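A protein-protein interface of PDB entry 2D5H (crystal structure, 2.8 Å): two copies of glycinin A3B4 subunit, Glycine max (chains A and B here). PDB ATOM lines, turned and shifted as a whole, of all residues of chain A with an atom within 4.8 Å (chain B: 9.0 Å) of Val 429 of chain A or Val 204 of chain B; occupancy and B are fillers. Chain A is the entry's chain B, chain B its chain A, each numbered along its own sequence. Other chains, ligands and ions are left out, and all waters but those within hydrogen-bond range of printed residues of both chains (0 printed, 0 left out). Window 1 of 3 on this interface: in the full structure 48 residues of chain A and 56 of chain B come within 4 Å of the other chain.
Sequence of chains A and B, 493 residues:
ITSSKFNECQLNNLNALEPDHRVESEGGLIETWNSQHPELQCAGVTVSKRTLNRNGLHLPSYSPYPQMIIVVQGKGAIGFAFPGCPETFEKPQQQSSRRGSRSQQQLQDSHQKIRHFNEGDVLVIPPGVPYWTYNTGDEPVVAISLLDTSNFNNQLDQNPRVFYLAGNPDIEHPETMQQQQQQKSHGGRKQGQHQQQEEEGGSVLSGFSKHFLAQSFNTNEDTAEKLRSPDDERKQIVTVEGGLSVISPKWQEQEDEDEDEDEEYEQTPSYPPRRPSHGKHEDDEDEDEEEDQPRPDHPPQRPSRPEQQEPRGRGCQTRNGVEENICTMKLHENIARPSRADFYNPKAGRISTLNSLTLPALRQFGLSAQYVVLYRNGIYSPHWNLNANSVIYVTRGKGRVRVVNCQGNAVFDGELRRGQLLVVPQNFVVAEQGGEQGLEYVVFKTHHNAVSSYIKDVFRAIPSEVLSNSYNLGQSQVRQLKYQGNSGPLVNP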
ATOM      1  N   PRO A 382       2.001   9.373 -22.110  1.00  0.00           N
ATOM      2  CA  PRO A 382       2.236   7.980 -21.722  1.00  0.00           C
ATOM      3  C   PRO A 382       2.932   7.153 -22.798  1.00  0.00           C
ATOM      4  O   PRO A 382       2.486   7.096 -23.945  1.00  0.00           O
ATOM      5  CB  PRO A 382       0.833   7.477 -21.409  1.00  0.00           C
ATOM      6  CG  PRO A 382       0.211   8.676 -20.780  1.00  0.00           C
ATOM      7  CD  PRO A 382       0.647   9.798 -21.710  1.00  0.00           C
ATOM      8  N   HIS A 383       4.031   6.517 -22.408  1.00  0.00           N
ATOM      9  CA  HIS A 383       4.816   5.686 -23.310  1.00  0.00           C
ATOM     10  C   HIS A 383       5.440   4.542 -22.517  1.00  0.00           C
ATOM     11  O   HIS A 383       5.089   4.325 -21.355  1.00  0.00           O
ATOM     12  CB  HIS A 383       5.908   6.525 -23.978  1.00  0.00           C
ATOM     13  CG  HIS A 383       6.782   7.259 -23.009  1.00  0.00           C
ATOM     14  ND1 HIS A 383       6.274   8.064 -22.011  1.00  0.00           N
ATOM     15  CD2 HIS A 383       8.129   7.319 -22.890  1.00  0.00           C
ATOM     16  CE1 HIS A 383       7.271   8.587 -21.318  1.00  0.00           C
ATOM     17  NE2 HIS A 383       8.407   8.150 -21.832  1.00  0.00           N
ATOM     18  N   TRP A 384       6.359   3.813 -23.144  1.00  0.00           N
ATOM     19  CA  TRP A 384       7.019   2.695 -22.479  1.00  0.00           C
ATOM     20  C   TRP A 384       8.219   2.200 -23.278  1.00  0.00           C
ATOM     21  O   TRP A 384       8.352   2.493 -24.468  1.00  0.00           O
ATOM     22  CB  TRP A 384       6.028   1.542 -22.284  1.00  0.00           C
ATOM     23  CG  TRP A 384       5.635   0.851 -23.568  1.00  0.00           C
ATOM     24  CD1 TRP A 384       6.393  -0.023 -24.297  1.00  0.00           C
ATOM     25  CD2 TRP A 384       4.402   1.000 -24.281  1.00  0.00           C
ATOM     26  NE1 TRP A 384       5.710  -0.425 -25.418  1.00  0.00           N
ATOM     27  CE2 TRP A 384       4.485   0.188 -25.434  1.00  0.00           C
ATOM     28  CE3 TRP A 384       3.234   1.744 -24.060  1.00  0.00           C
ATOM     29  CZ2 TRP A 384       3.444   0.096 -26.363  1.00  0.00           C
ATOM     30  CZ3 TRP A 384       2.199   1.652 -24.986  1.00  0.00           C
ATOM     31  CH2 TRP A 384       2.314   0.834 -26.124  1.00  0.00           C
ATOM     32  N   ARG A 402       3.895   9.220 -13.143  1.00  0.00           N
ATOM     33  CA  ARG A 402       2.945   8.117 -13.134  1.00  0.00           C
ATOM     34  C   ARG A 402       3.512   6.905 -13.865  1.00  0.00           C
ATOM     35  O   ARG A 402       3.940   7.006 -15.018  1.00  0.00           O
ATOM     36  CB  ARG A 402       1.630   8.554 -13.787  1.00  0.00           C
ATOM     37  CG  ARG A 402       0.741   9.407 -12.888  1.00  0.00           C
ATOM     38  CD  ARG A 402      -0.436   9.996 -13.658  1.00  0.00           C
ATOM     39  NE  ARG A 402      -1.523  10.431 -12.780  1.00  0.00           N
ATOM     40  CZ  ARG A 402      -1.390  11.301 -11.784  1.00  0.00           C
ATOM     41  NH1 ARG A 402      -0.209  11.844 -11.520  1.00  0.00           N
ATOM     42  NH2 ARG A 402      -2.443  11.629 -11.047  1.00  0.00           N
ATOM     43  N   VAL A 403       3.520   5.763 -13.185  1.00  0.00           N
ATOM     44  CA  VAL A 403       4.030   4.530 -13.769  1.00  0.00           C
ATOM     45  C   VAL A 403       3.004   3.413 -13.613  1.00  0.00           C
ATOM     46  O   VAL A 403       2.712   2.973 -12.499  1.00  0.00           O
ATOM     47  CB  VAL A 403       5.346   4.102 -13.097  1.00  0.00           C
ATOM     48  CG1 VAL A 403       5.895   2.862 -13.778  1.00  0.00           C
ATOM     49  CG2 VAL A 403       6.352   5.239 -13.163  1.00  0.00           C
ATOM     50  N   VAL A 404       2.464   2.958 -14.740  1.00  0.00           N
ATOM     51  CA  VAL A 404       1.456   1.905 -14.744  1.00  0.00           C
ATOM     52  C   VAL A 404       2.042   0.542 -15.107  1.00  0.00           C
ATOM     53  O   VAL A 404       2.830   0.425 -16.047  1.00  0.00           O
ATOM     54  CB  VAL A 404       0.323   2.241 -15.737  1.00  0.00           C
ATOM     55  CG1 VAL A 404      -0.752   1.164 -15.690  1.00  0.00           C
ATOM     56  CG2 VAL A 404      -0.267   3.605 -15.402  1.00  0.00           C
ATOM     57  N   GLY A 408      -2.554  -2.851 -15.060  1.00  0.00           N
ATOM     58  CA  GLY A 408      -3.351  -1.646 -15.193  1.00  0.00           C
ATOM     59  C   GLY A 408      -3.408  -0.848 -13.904  1.00  0.00           C
ATOM     60  O   GLY A 408      -4.406  -0.182 -13.624  1.00  0.00           O
ATOM     61  N   ASN A 427       8.612  -2.913 -19.942  1.00  0.00           N
ATOM     62  CA  ASN A 427       7.339  -2.611 -20.587  1.00  0.00           C
ATOM     63  C   ASN A 427       6.377  -1.725 -19.805  1.00  0.00           C
ATOM     64  O   ASN A 427       5.339  -1.329 -20.336  1.00  0.00           O
ATOM     65  CB  ASN A 427       6.630  -3.909 -20.985  1.00  0.00           C
ATOM     66  CG  ASN A 427       7.168  -4.489 -22.278  1.00  0.00           C
ATOM     67  OD1 ASN A 427       6.727  -5.544 -22.724  1.00  0.00           O
ATOM     68  ND2 ASN A 427       8.121  -3.796 -22.892  1.00  0.00           N
ATOM     69  N   PHE A 428       6.709  -1.413 -18.555  1.00  0.00           N
ATOM     70  CA  PHE A 428       5.838  -0.557 -17.756  1.00  0.00           C
ATOM     71  C   PHE A 428       5.572   0.747 -18.501  1.00  0.00           C
ATOM     72  O   PHE A 428       6.419   1.227 -19.255  1.00  0.00           O
ATOM     73  CB  PHE A 428       6.466  -0.251 -16.392  1.00  0.00           C
ATOM     74  CG  PHE A 428       6.397  -1.392 -15.415  1.00  0.00           C
ATOM     75  CD1 PHE A 428       6.172  -1.149 -14.064  1.00  0.00           C
ATOM     76  CD2 PHE A 428       6.569  -2.707 -15.836  1.00  0.00           C
ATOM     77  CE1 PHE A 428       6.117  -2.193 -13.145  1.00  0.00           C
ATOM     78  CE2 PHE A 428       6.518  -3.762 -14.925  1.00  0.00           C
ATOM     79  CZ  PHE A 428       6.290  -3.503 -13.575  1.00  0.00           C
ATOM     80  N   VAL A 429       4.387   1.313 -18.294  1.00  0.00           N
ATOM     81  CA  VAL A 429       4.018   2.561 -18.948  1.00  0.00           C
ATOM     82  C   VAL A 429       4.351   3.737 -18.039  1.00  0.00           C
ATOM     83  O   VAL A 429       3.857   3.823 -16.914  1.00  0.00           O
ATOM     84  CB  VAL A 429       2.514   2.595 -19.279  1.00  0.00           C
ATOM     85  CG1 VAL A 429       2.185   3.853 -20.076  1.00  0.00           C
ATOM     86  CG2 VAL A 429       2.128   1.349 -20.059  1.00  0.00           C
ATOM     87  N   VAL A 430       5.186   4.642 -18.530  1.00  0.00           N
ATOM     88  CA  VAL A 430       5.582   5.800 -17.744  1.00  0.00           C
ATOM     89  C   VAL A 430       5.065   7.107 -18.331  1.00  0.00           C
ATOM     90  O   VAL A 430       5.214   7.375 -19.526  1.00  0.00           O
ATOM     91  CB  VAL A 430       7.120   5.891 -17.614  1.00  0.00           C
ATOM     92  CG1 VAL A 430       7.756   6.002 -18.993  1.00  0.00           C
ATOM     93  CG2 VAL A 430       7.499   7.084 -16.750  1.00  0.00           C
ATOM     94  N   ALA A 431       4.457   7.917 -17.472  1.00  0.00           N
ATOM     95  CA  ALA A 431       3.920   9.211 -17.870  1.00  0.00           C
ATOM     96  C   ALA A 431       4.209  10.202 -16.751  1.00  0.00           C
ATOM     97  O   ALA A 431       3.995   9.899 -15.577  1.00  0.00           O
ATOM     98  CB  ALA A 431       2.417   9.107 -18.111  1.00  0.00           C
ATOM     99  N   ILE A 455       1.715   5.541 -26.506  1.00  0.00           N
ATOM    100  CA  ILE A 455       0.343   5.146 -26.809  1.00  0.00           C
ATOM    101  C   ILE A 455      -0.269   5.859 -28.006  1.00  0.00           C
ATOM    102  O   ILE A 455      -0.807   5.215 -28.908  1.00  0.00           O
ATOM    103  CB  ILE A 455      -0.573   5.373 -25.593  1.00  0.00           C
ATOM    104  CG1 ILE A 455      -0.060   4.564 -24.401  1.00  0.00           C
ATOM    105  CG2 ILE A 455      -2.003   4.972 -25.934  1.00  0.00           C
ATOM    106  CD1 ILE A 455      -0.836   4.795 -23.121  1.00  0.00           C
ATOM    107  N   PRO B  60      -5.648  -5.390 -28.466  1.00  0.00           N
ATOM    108  CA  PRO B  60      -4.209  -5.129 -28.556  1.00  0.00           C
ATOM    109  C   PRO B  60      -3.481  -5.303 -27.223  1.00  0.00           C
ATOM    110  O   PRO B  60      -4.062  -5.105 -26.154  1.00  0.00           O
ATOM    111  CB  PRO B  60      -4.159  -3.695 -29.072  1.00  0.00           C
ATOM    112  CG  PRO B  60      -5.344  -3.647 -29.983  1.00  0.00           C
ATOM    113  CD  PRO B  60      -6.412  -4.335 -29.159  1.00  0.00           C
ATOM    114  N   SER B  61      -2.208  -5.682 -27.302  1.00  0.00           N
ATOM    115  CA  SER B  61      -1.387  -5.888 -26.115  1.00  0.00           C
ATOM    116  C   SER B  61       0.060  -6.169 -26.510  1.00  0.00           C
ATOM    117  O   SER B  61       0.370  -6.330 -27.690  1.00  0.00           O
ATOM    118  CB  SER B  61      -1.928  -7.062 -25.299  1.00  0.00           C
ATOM    119  OG  SER B  61      -1.881  -8.260 -26.054  1.00  0.00           O
ATOM    120  N   TYR B  62       0.939  -6.219 -25.514  1.00  0.00           N
ATOM    121  CA  TYR B  62       2.352  -6.494 -25.747  1.00  0.00           C
ATOM    122  C   TYR B  62       2.968  -7.157 -24.517  1.00  0.00           C
ATOM    123  O   TYR B  62       2.498  -6.962 -23.394  1.00  0.00           O
ATOM    124  CB  TYR B  62       3.107  -5.202 -26.079  1.00  0.00           C
ATOM    125  CG  TYR B  62       2.989  -4.123 -25.028  1.00  0.00           C
ATOM    126  CD1 TYR B  62       1.813  -3.388 -24.881  1.00  0.00           C
ATOM    127  CD2 TYR B  62       4.053  -3.840 -24.171  1.00  0.00           C
ATOM    128  CE1 TYR B  62       1.700  -2.395 -23.909  1.00  0.00           C
ATOM    129  CE2 TYR B  62       3.949  -2.851 -23.194  1.00  0.00           C
ATOM    130  CZ  TYR B  62       2.770  -2.133 -23.069  1.00  0.00           C
ATOM    131  OH  TYR B  62       2.659  -1.162 -22.101  1.00  0.00           O
ATOM    132  N   PRO B 130       2.870  -3.814 -29.516  1.00  0.00           N
ATOM    133  CA  PRO B 130       1.433  -4.067 -29.347  1.00  0.00           C
ATOM    134  C   PRO B 130       0.867  -4.791 -30.572  1.00  0.00           C
ATOM    135  O   PRO B 130       1.335  -4.575 -31.692  1.00  0.00           O
ATOM    136  CB  PRO B 130       0.845  -2.663 -29.198  1.00  0.00           C
ATOM    137  CG  PRO B 130       2.004  -1.843 -28.701  1.00  0.00           C
ATOM    138  CD  PRO B 130       3.137  -2.366 -29.535  1.00  0.00           C
ATOM    139  N   VAL B 162       1.335  -9.460 -19.643  1.00  0.00           N
ATOM    140  CA  VAL B 162       0.640  -8.947 -20.817  1.00  0.00           C
ATOM    141  C   VAL B 162       0.045  -7.579 -20.508  1.00  0.00           C
ATOM    142  O   VAL B 162      -0.685  -7.418 -19.528  1.00  0.00           O
ATOM    143  CB  VAL B 162      -0.499  -9.892 -21.260  1.00  0.00           C
ATOM    144  CG1 VAL B 162      -1.187  -9.333 -22.499  1.00  0.00           C
ATOM    145  CG2 VAL B 162       0.054 -11.279 -21.538  1.00  0.00           C
ATOM    146  N   PHE B 163       0.362  -6.599 -21.346  1.00  0.00           N
ATOM    147  CA  PHE B 163      -0.141  -5.244 -21.161  1.00  0.00           C
ATOM    148  C   PHE B 163      -1.226  -4.934 -22.189  1.00  0.00           C
ATOM    149  O   PHE B 163      -0.937  -4.781 -23.377  1.00  0.00           O
ATOM    150  CB  PHE B 163       0.996  -4.228 -21.312  1.00  0.00           C
ATOM    151  CG  PHE B 163       2.128  -4.415 -20.337  1.00  0.00           C
ATOM    152  CD1 PHE B 163       2.879  -5.586 -20.331  1.00  0.00           C
ATOM    153  CD2 PHE B 163       2.457  -3.409 -19.437  1.00  0.00           C
ATOM    154  CE1 PHE B 163       3.939  -5.753 -19.443  1.00  0.00           C
ATOM    155  CE2 PHE B 163       3.517  -3.566 -18.545  1.00  0.00           C
ATOM    156  CZ  PHE B 163       4.258  -4.740 -18.549  1.00  0.00           C
ATOM    157  N   TYR B 164      -2.473  -4.846 -21.737  1.00  0.00           N
ATOM    158  CA  TYR B 164      -3.579  -4.541 -22.635  1.00  0.00           C
ATOM    159  C   TYR B 164      -3.815  -3.043 -22.750  1.00  0.00           C
ATOM    160  O   TYR B 164      -3.695  -2.311 -21.770  1.00  0.00           O
ATOM    161  CB  TYR B 164      -4.866  -5.219 -22.166  1.00  0.00           C
ATOM    162  CG  TYR B 164      -4.978  -6.662 -22.592  1.00  0.00           C
ATOM    163  CD1 TYR B 164      -4.484  -7.691 -21.791  1.00  0.00           C
ATOM    164  CD2 TYR B 164      -5.555  -6.998 -23.817  1.00  0.00           C
ATOM    165  CE1 TYR B 164      -4.564  -9.019 -22.199  1.00  0.00           C
ATOM    166  CE2 TYR B 164      -5.635  -8.321 -24.234  1.00  0.00           C
ATOM    167  CZ  TYR B 164      -5.139  -9.326 -23.422  1.00  0.00           C
ATOM    168  OH  TYR B 164      -5.222 -10.634 -23.836  1.00  0.00           O
ATOM    169  N   LEU B 165      -4.153  -2.593 -23.953  1.00  0.00           N
ATOM    170  CA  LEU B 165      -4.409  -1.181 -24.191  1.00  0.00           C
ATOM    171  C   LEU B 165      -5.878  -0.813 -23.997  1.00  0.00           C
ATOM    172  O   LEU B 165      -6.216   0.368 -23.921  1.00  0.00           O
ATOM    173  CB  LEU B 165      -3.970  -0.795 -25.605  1.00  0.00           C
ATOM    174  CG  LEU B 165      -2.476  -0.908 -25.924  1.00  0.00           C
ATOM    175  CD1 LEU B 165      -2.231  -0.476 -27.366  1.00  0.00           C
ATOM    176  CD2 LEU B 165      -1.669  -0.034 -24.966  1.00  0.00           C
ATOM    177  N   ALA B 166      -6.748  -1.817 -23.912  1.00  0.00           N
ATOM    178  CA  ALA B 166      -8.175  -1.565 -23.732  1.00  0.00           C
ATOM    179  C   ALA B 166      -8.917  -2.716 -23.057  1.00  0.00           C
ATOM    180  O   ALA B 166      -8.492  -3.869 -23.127  1.00  0.00           O
ATOM    181  CB  ALA B 166      -8.819  -1.263 -25.081  1.00  0.00           C
ATOM    182  N   GLY B 167     -10.029  -2.382 -22.404  1.00  0.00           N
ATOM    183  CA  GLY B 167     -10.846  -3.380 -21.736  1.00  0.00           C
ATOM    184  C   GLY B 167     -10.445  -3.730 -20.314  1.00  0.00           C
ATOM    185  O   GLY B 167      -9.394  -3.318 -19.828  1.00  0.00           O
ATOM    186  N   ASN B 168     -11.305  -4.496 -19.647  1.00  0.00           N
ATOM    187  CA  ASN B 168     -11.064  -4.943 -18.278  1.00  0.00           C
ATOM    188  C   ASN B 168     -10.932  -6.471 -18.323  1.00  0.00           C
ATOM    189  O   ASN B 168     -11.865  -7.203 -17.975  1.00  0.00           O
ATOM    190  CB  ASN B 168     -12.234  -4.534 -17.376  1.00  0.00           C
ATOM    191  CG  ASN B 168     -12.036  -4.957 -15.930  1.00  0.00           C
ATOM    192  OD1 ASN B 168     -11.084  -4.538 -15.270  1.00  0.00           O
ATOM    193  ND2 ASN B 168     -12.943  -5.789 -15.430  1.00  0.00           N
ATOM    194  N   PRO B 169      -9.760  -6.966 -18.757  1.00  0.00           N
ATOM    195  CA  PRO B 169      -9.456  -8.395 -18.876  1.00  0.00           C
ATOM    196  C   PRO B 169      -9.261  -9.147 -17.569  1.00  0.00           C
ATOM    197  O   PRO B 169      -9.122  -8.551 -16.501  1.00  0.00           O
ATOM    198  CB  PRO B 169      -8.188  -8.397 -19.718  1.00  0.00           C
ATOM    199  CG  PRO B 169      -7.481  -7.188 -19.204  1.00  0.00           C
ATOM    200  CD  PRO B 169      -8.593  -6.158 -19.160  1.00  0.00           C
ATOM    201  N   GLY B 201      -7.708  -6.679 -12.780  1.00  0.00           N
ATOM    202  CA  GLY B 201      -6.953  -6.379 -13.984  1.00  0.00           C
ATOM    203  C   GLY B 201      -7.124  -4.968 -14.510  1.00  0.00           C
ATOM    204  O   GLY B 201      -7.188  -4.006 -13.742  1.00  0.00           O
ATOM    205  N   GLY B 202      -7.191  -4.848 -15.833  1.00  0.00           N
ATOM    206  CA  GLY B 202      -7.355  -3.548 -16.456  1.00  0.00           C
ATOM    207  C   GLY B 202      -6.260  -3.247 -17.460  1.00  0.00           C
ATOM    208  O   GLY B 202      -5.147  -3.758 -17.345  1.00  0.00           O
ATOM    209  N   SER B 203      -6.578  -2.424 -18.454  1.00  0.00           N
ATOM    210  CA  SER B 203      -5.605  -2.047 -19.469  1.00  0.00           C
ATOM    211  C   SER B 203      -4.614  -1.088 -18.828  1.00  0.00           C
ATOM    212  O   SER B 203      -4.846  -0.602 -17.721  1.00  0.00           O
ATOM    213  CB  SER B 203      -6.297  -1.356 -20.646  1.00  0.00           C
ATOM    214  OG  SER B 203      -6.892  -0.131 -20.246  1.00  0.00           O
ATOM    215  N   VAL B 204      -3.512  -0.812 -19.516  1.00  0.00           N
ATOM    216  CA  VAL B 204      -2.512   0.099 -18.977  1.00  0.00           C
ATOM    217  C   VAL B 204      -3.146   1.453 -18.684  1.00  0.00           C
ATOM    218  O   VAL B 204      -2.791   2.115 -17.711  1.00  0.00           O
ATOM    219  CB  VAL B 204      -1.338   0.302 -19.961  1.00  0.00           C
ATOM    220  CG1 VAL B 204      -0.650  -1.028 -20.229  1.00  0.00           C
ATOM    221  CG2 VAL B 204      -1.838   0.919 -21.257  1.00  0.00           C
ATOM    222  N   LEU B 205      -4.103   1.844 -19.519  1.00  0.00           N
ATOM    223  CA  LEU B 205      -4.785   3.125 -19.372  1.00  0.00           C
ATOM    224  C   LEU B 205      -5.738   3.207 -18.180  1.00  0.00           C
ATOM    225  O   LEU B 205      -6.021   4.301 -17.688  1.00  0.00           O
ATOM    226  CB  LEU B 205      -5.542   3.460 -20.660  1.00  0.00           C
ATOM    227  CG  LEU B 205      -4.666   3.713 -21.890  1.00  0.00           C
ATOM    228  CD1 LEU B 205      -5.534   3.892 -23.123  1.00  0.00           C
ATOM    229  CD2 LEU B 205      -3.809   4.942 -21.654  1.00  0.00           C
ATOM    230  N   SER B 206      -6.229   2.066 -17.708  1.00  0.00           N
ATOM    231  CA  SER B 206      -7.146   2.068 -16.571  1.00  0.00           C
ATOM    232  C   SER B 206      -6.476   2.680 -15.343  1.00  0.00           C
ATOM    233  O   SER B 206      -7.138   3.000 -14.355  1.00  0.00           O
ATOM    234  CB  SER B 206      -7.615   0.644 -16.245  1.00  0.00           C
ATOM    235  OG  SER B 206      -6.581  -0.126 -15.657  1.00  0.00           O
ATOM    236  N   GLY B 207      -5.159   2.838 -15.412  1.00  0.00           N
ATOM    237  CA  GLY B 207      -4.429   3.414 -14.299  1.00  0.00           C
ATOM    238  C   GLY B 207      -4.410   4.928 -14.368  1.00  0.00           C
ATOM    239  O   GLY B 207      -4.352   5.604 -13.340  1.00  0.00           O
ATOM    240  N   PHE B 208      -4.463   5.459 -15.585  1.00  0.00           N
ATOM    241  CA  PHE B 208      -4.454   6.901 -15.798  1.00  0.00           C
ATOM    242  C   PHE B 208      -5.848   7.513 -15.670  1.00  0.00           C
ATOM    243  O   PHE B 208      -6.816   6.999 -16.233  1.00  0.00           O
ATOM    244  CB  PHE B 208      -3.885   7.231 -17.182  1.00  0.00           C
ATOM    245  CG  PHE B 208      -2.419   6.930 -17.328  1.00  0.00           C
ATOM    246  CD1 PHE B 208      -1.495   7.443 -16.421  1.00  0.00           C
ATOM    247  CD2 PHE B 208      -1.956   6.161 -18.389  1.00  0.00           C
ATOM    248  CE1 PHE B 208      -0.132   7.194 -16.570  1.00  0.00           C
ATOM    249  CE2 PHE B 208      -0.593   5.906 -18.546  1.00  0.00           C
ATOM    250  CZ  PHE B 208       0.319   6.424 -17.635  1.00  0.00           C
ATOM    251  N   SER B 209      -5.939   8.613 -14.929  1.00  0.00           N
ATOM    252  CA  SER B 209      -7.208   9.307 -14.733  1.00  0.00           C
ATOM    253  C   SER B 209      -7.575  10.069 -16.005  1.00  0.00           C
ATOM    254  O   SER B 209      -6.697  10.560 -16.718  1.00  0.00           O
ATOM    255  CB  SER B 209      -7.102  10.275 -13.550  1.00  0.00           C
ATOM    256  OG  SER B 209      -6.043  11.199 -13.735  1.00  0.00           O
ATOM    257  N   LEU B 213      -5.089  11.983 -18.695  1.00  0.00           N
ATOM    258  CA  LEU B 213      -5.255  11.306 -19.977  1.00  0.00           C
ATOM    259  C   LEU B 213      -5.850  12.237 -21.030  1.00  0.00           C
ATOM    260  O   LEU B 213      -5.294  12.396 -22.119  1.00  0.00           O
ATOM    261  CB  LEU B 213      -6.150  10.077 -19.804  1.00  0.00           C
ATOM    262  CG  LEU B 213      -6.330   9.156 -21.013  1.00  0.00           C
ATOM    263  CD1 LEU B 213      -4.979   8.662 -21.502  1.00  0.00           C
ATOM    264  CD2 LEU B 213      -7.209   7.982 -20.621  1.00  0.00           C
ATOM    265  N   PHE B 217      -3.543  13.239 -24.361  1.00  0.00           N
ATOM    266  CA  PHE B 217      -3.989  13.001 -25.730  1.00  0.00           C
ATOM    267  C   PHE B 217      -4.891  14.120 -26.237  1.00  0.00           C
ATOM    268  O   PHE B 217      -5.652  13.929 -27.184  1.00  0.00           O
ATOM    269  CB  PHE B 217      -4.728  11.663 -25.822  1.00  0.00           C
ATOM    270  CG  PHE B 217      -3.883  10.478 -25.453  1.00  0.00           C
ATOM    271  CD1 PHE B 217      -3.495  10.266 -24.134  1.00  0.00           C
ATOM    272  CD2 PHE B 217      -3.461   9.580 -26.424  1.00  0.00           C
ATOM    273  CE1 PHE B 217      -2.699   9.179 -23.790  1.00  0.00           C
ATOM    274  CE2 PHE B 217      -2.663   8.487 -26.088  1.00  0.00           C
ATOM    275  CZ  PHE B 217      -2.283   8.289 -24.767  1.00  0.00           C
ATOM    276  N   LEU B 227     -11.532   5.495 -22.693  1.00  0.00           N
ATOM    277  CA  LEU B 227     -10.217   4.910 -22.942  1.00  0.00           C
ATOM    278  C   LEU B 227      -9.721   4.109 -21.741  1.00  0.00           C
ATOM    279  O   LEU B 227      -8.759   3.349 -21.845  1.00  0.00           O
ATOM    280  CB  LEU B 227      -9.207   6.007 -23.298  1.00  0.00           C
ATOM    281  CG  LEU B 227      -9.443   6.728 -24.632  1.00  0.00           C
ATOM    282  CD1 LEU B 227      -8.424   7.844 -24.811  1.00  0.00           C
ATOM    283  CD2 LEU B 227      -9.346   5.730 -25.777  1.00  0.00           C
ATOM    284  N   ARG B 228     -10.382   4.288 -20.602  1.00  0.00           N
ATOM    285  CA  ARG B 228     -10.034   3.560 -19.387  1.00  0.00           C
ATOM    286  C   ARG B 228     -10.868   2.284 -19.364  1.00  0.00           C
ATOM    287  O   ARG B 228     -10.703   1.423 -18.495  1.00  0.00           O
ATOM    288  CB  ARG B 228     -10.346   4.405 -18.149  1.00  0.00           C
ATOM    289  CG  ARG B 228      -9.480   5.647 -18.001  1.00  0.00           C
ATOM    290  CD  ARG B 228      -9.896   6.504 -16.806  1.00  0.00           C
ATOM    291  NE  ARG B 228      -9.918   5.761 -15.546  1.00  0.00           N
ATOM    292  CZ  ARG B 228     -10.937   5.011 -15.130  1.00  0.00           C
ATOM    293  NH1 ARG B 228     -12.031   4.900 -15.871  1.00  0.00           N
ATOM    294  NH2 ARG B 228     -10.860   4.371 -13.971  1.00  0.00           N
ATOM    295  N   SER B 229     -11.773   2.187 -20.335  1.00  0.00           N
ATOM    296  CA  SER B 229     -12.662   1.041 -20.486  1.00  0.00           C
ATOM    297  C   SER B 229     -13.328   0.590 -19.186  1.00  0.00           C
ATOM    298  O   SER B 229     -13.342  -0.602 -18.874  1.00  0.00           O
ATOM    299  CB  SER B 229     -11.895  -0.131 -21.103  1.00  0.00           C
ATOM    300  OG  SER B 229     -11.360   0.226 -22.367  1.00  0.00           O
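Phe 217 of chain B touches Pro 382 of chain A.
CZ2 of Trp 384 of chain A touches CG of Pro 130 of chain B, 3.4 Å away.
Val 204 of chain B touches Val 404 of chain A (O to CG1, 3.0 Å).
Phe 208 of chain B touches Val 404 of chain A.
Gly 408 of chain A touches Gly 202 of chain B (CA to O, 3.5 Å).
Gly 408 of chain A touches Ser 203 of chain B (CA to O, 3.1 Å).
Phe 163 of chain B touches Asn 427 of chain A (CE2 to O, 3.4 Å).
Phe 163 of chain B touches Phe 428 of chain A (CE2 to N, 3.9 Å).
CG1 of Val 429 of chain A touches CE2 of Phe 208 of chain B, 3.8 Å away.
CB of Ile 455 of chain A touches CZ of Phe 217 of chain B (3.5 Å).
Of the 13 printed residues of chain A, 10 touch a printed residue of chain B.
Along chain A the printed residues that touch a printed residue of chain B span positions 382 to 455.
Of the 26 printed residues of chain B, 11 touch a printed residue of chain A.
Printed residues of chain B that touch a printed residue of chain A: Tyr 62, Pro 130, Phe 163, Gly 202, Ser 203, Val 204, Leu 205, Ser 206, Gly 207, Phe 208 and Phe 217.
N of Phe 163 of chain B is in hydrogen-bond range of O of Tyr 62 of chain B (3.0 Å).
O of Tyr 164 of chain B sits at hydrogen-bond distance from N of Val 204 of chain B, 2.7 Å away.
O of Gly 167 of chain B lies within hydrogen-bond range of N of Ser 203 of chain B (3.3 Å).
The backbone carbonyl oxygen (O) of Ser 203 of chain B is in hydrogen-bond range of the side-chain hydroxyl (OG) of Ser 206 of chain B (2.7 Å).
N of Arg 402 of chain A is in hydrogen-bond range of O of Ala 431 of chain A.
The backbone NH of Val 404 of chain A lies within hydrogen-bond range of the backbone carbonyl oxygen of Val 429 of chain A, at 2.7 Å.
O of Asn 427 of chain A sits at hydrogen-bond distance from OH of Tyr 62 of chain B, at 3.2 Å.
OG of Ser 206 of chain B is in hydrogen-bond range of O of Gly 408 of chain A (3.0 Å).
No position is printed for both chains.
Val 404 of chain A touches two residues of chain B.
Val 429 of chain A touches just these residues of chain B: Tyr 62, Val 204 and Phe 208.
No residue of chain B comes within 4 Å of Val 430 of chain A.
Of chain A, only Val 404 and Val 429 come within 4 Å of Val 204 of chain B.
Printed residues of chain A within 4 Å of Ser 206 of chain B: Gly 408 (3.0 Å).
Of the printed residues of chain A, Gly 207 of chain B touches Gly 408 (3.6 Å).
Of the printed residues of chain A, Phe 208 of chain B touches Pro 382 (3.6 Å), Arg 402 (3.6 Å), Val 404 (3.6 Å), Val 429 (3.8 Å) and Ala 431 (3.4 Å).
The nearest residue of chain A that does not touch Val 204 of chain B is Gly 408 of chain A (4.3 Å).
The nearest printed residue of chain A that does not touch Gly 202 of chain B is Val 404 of chain A (6.8 Å).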
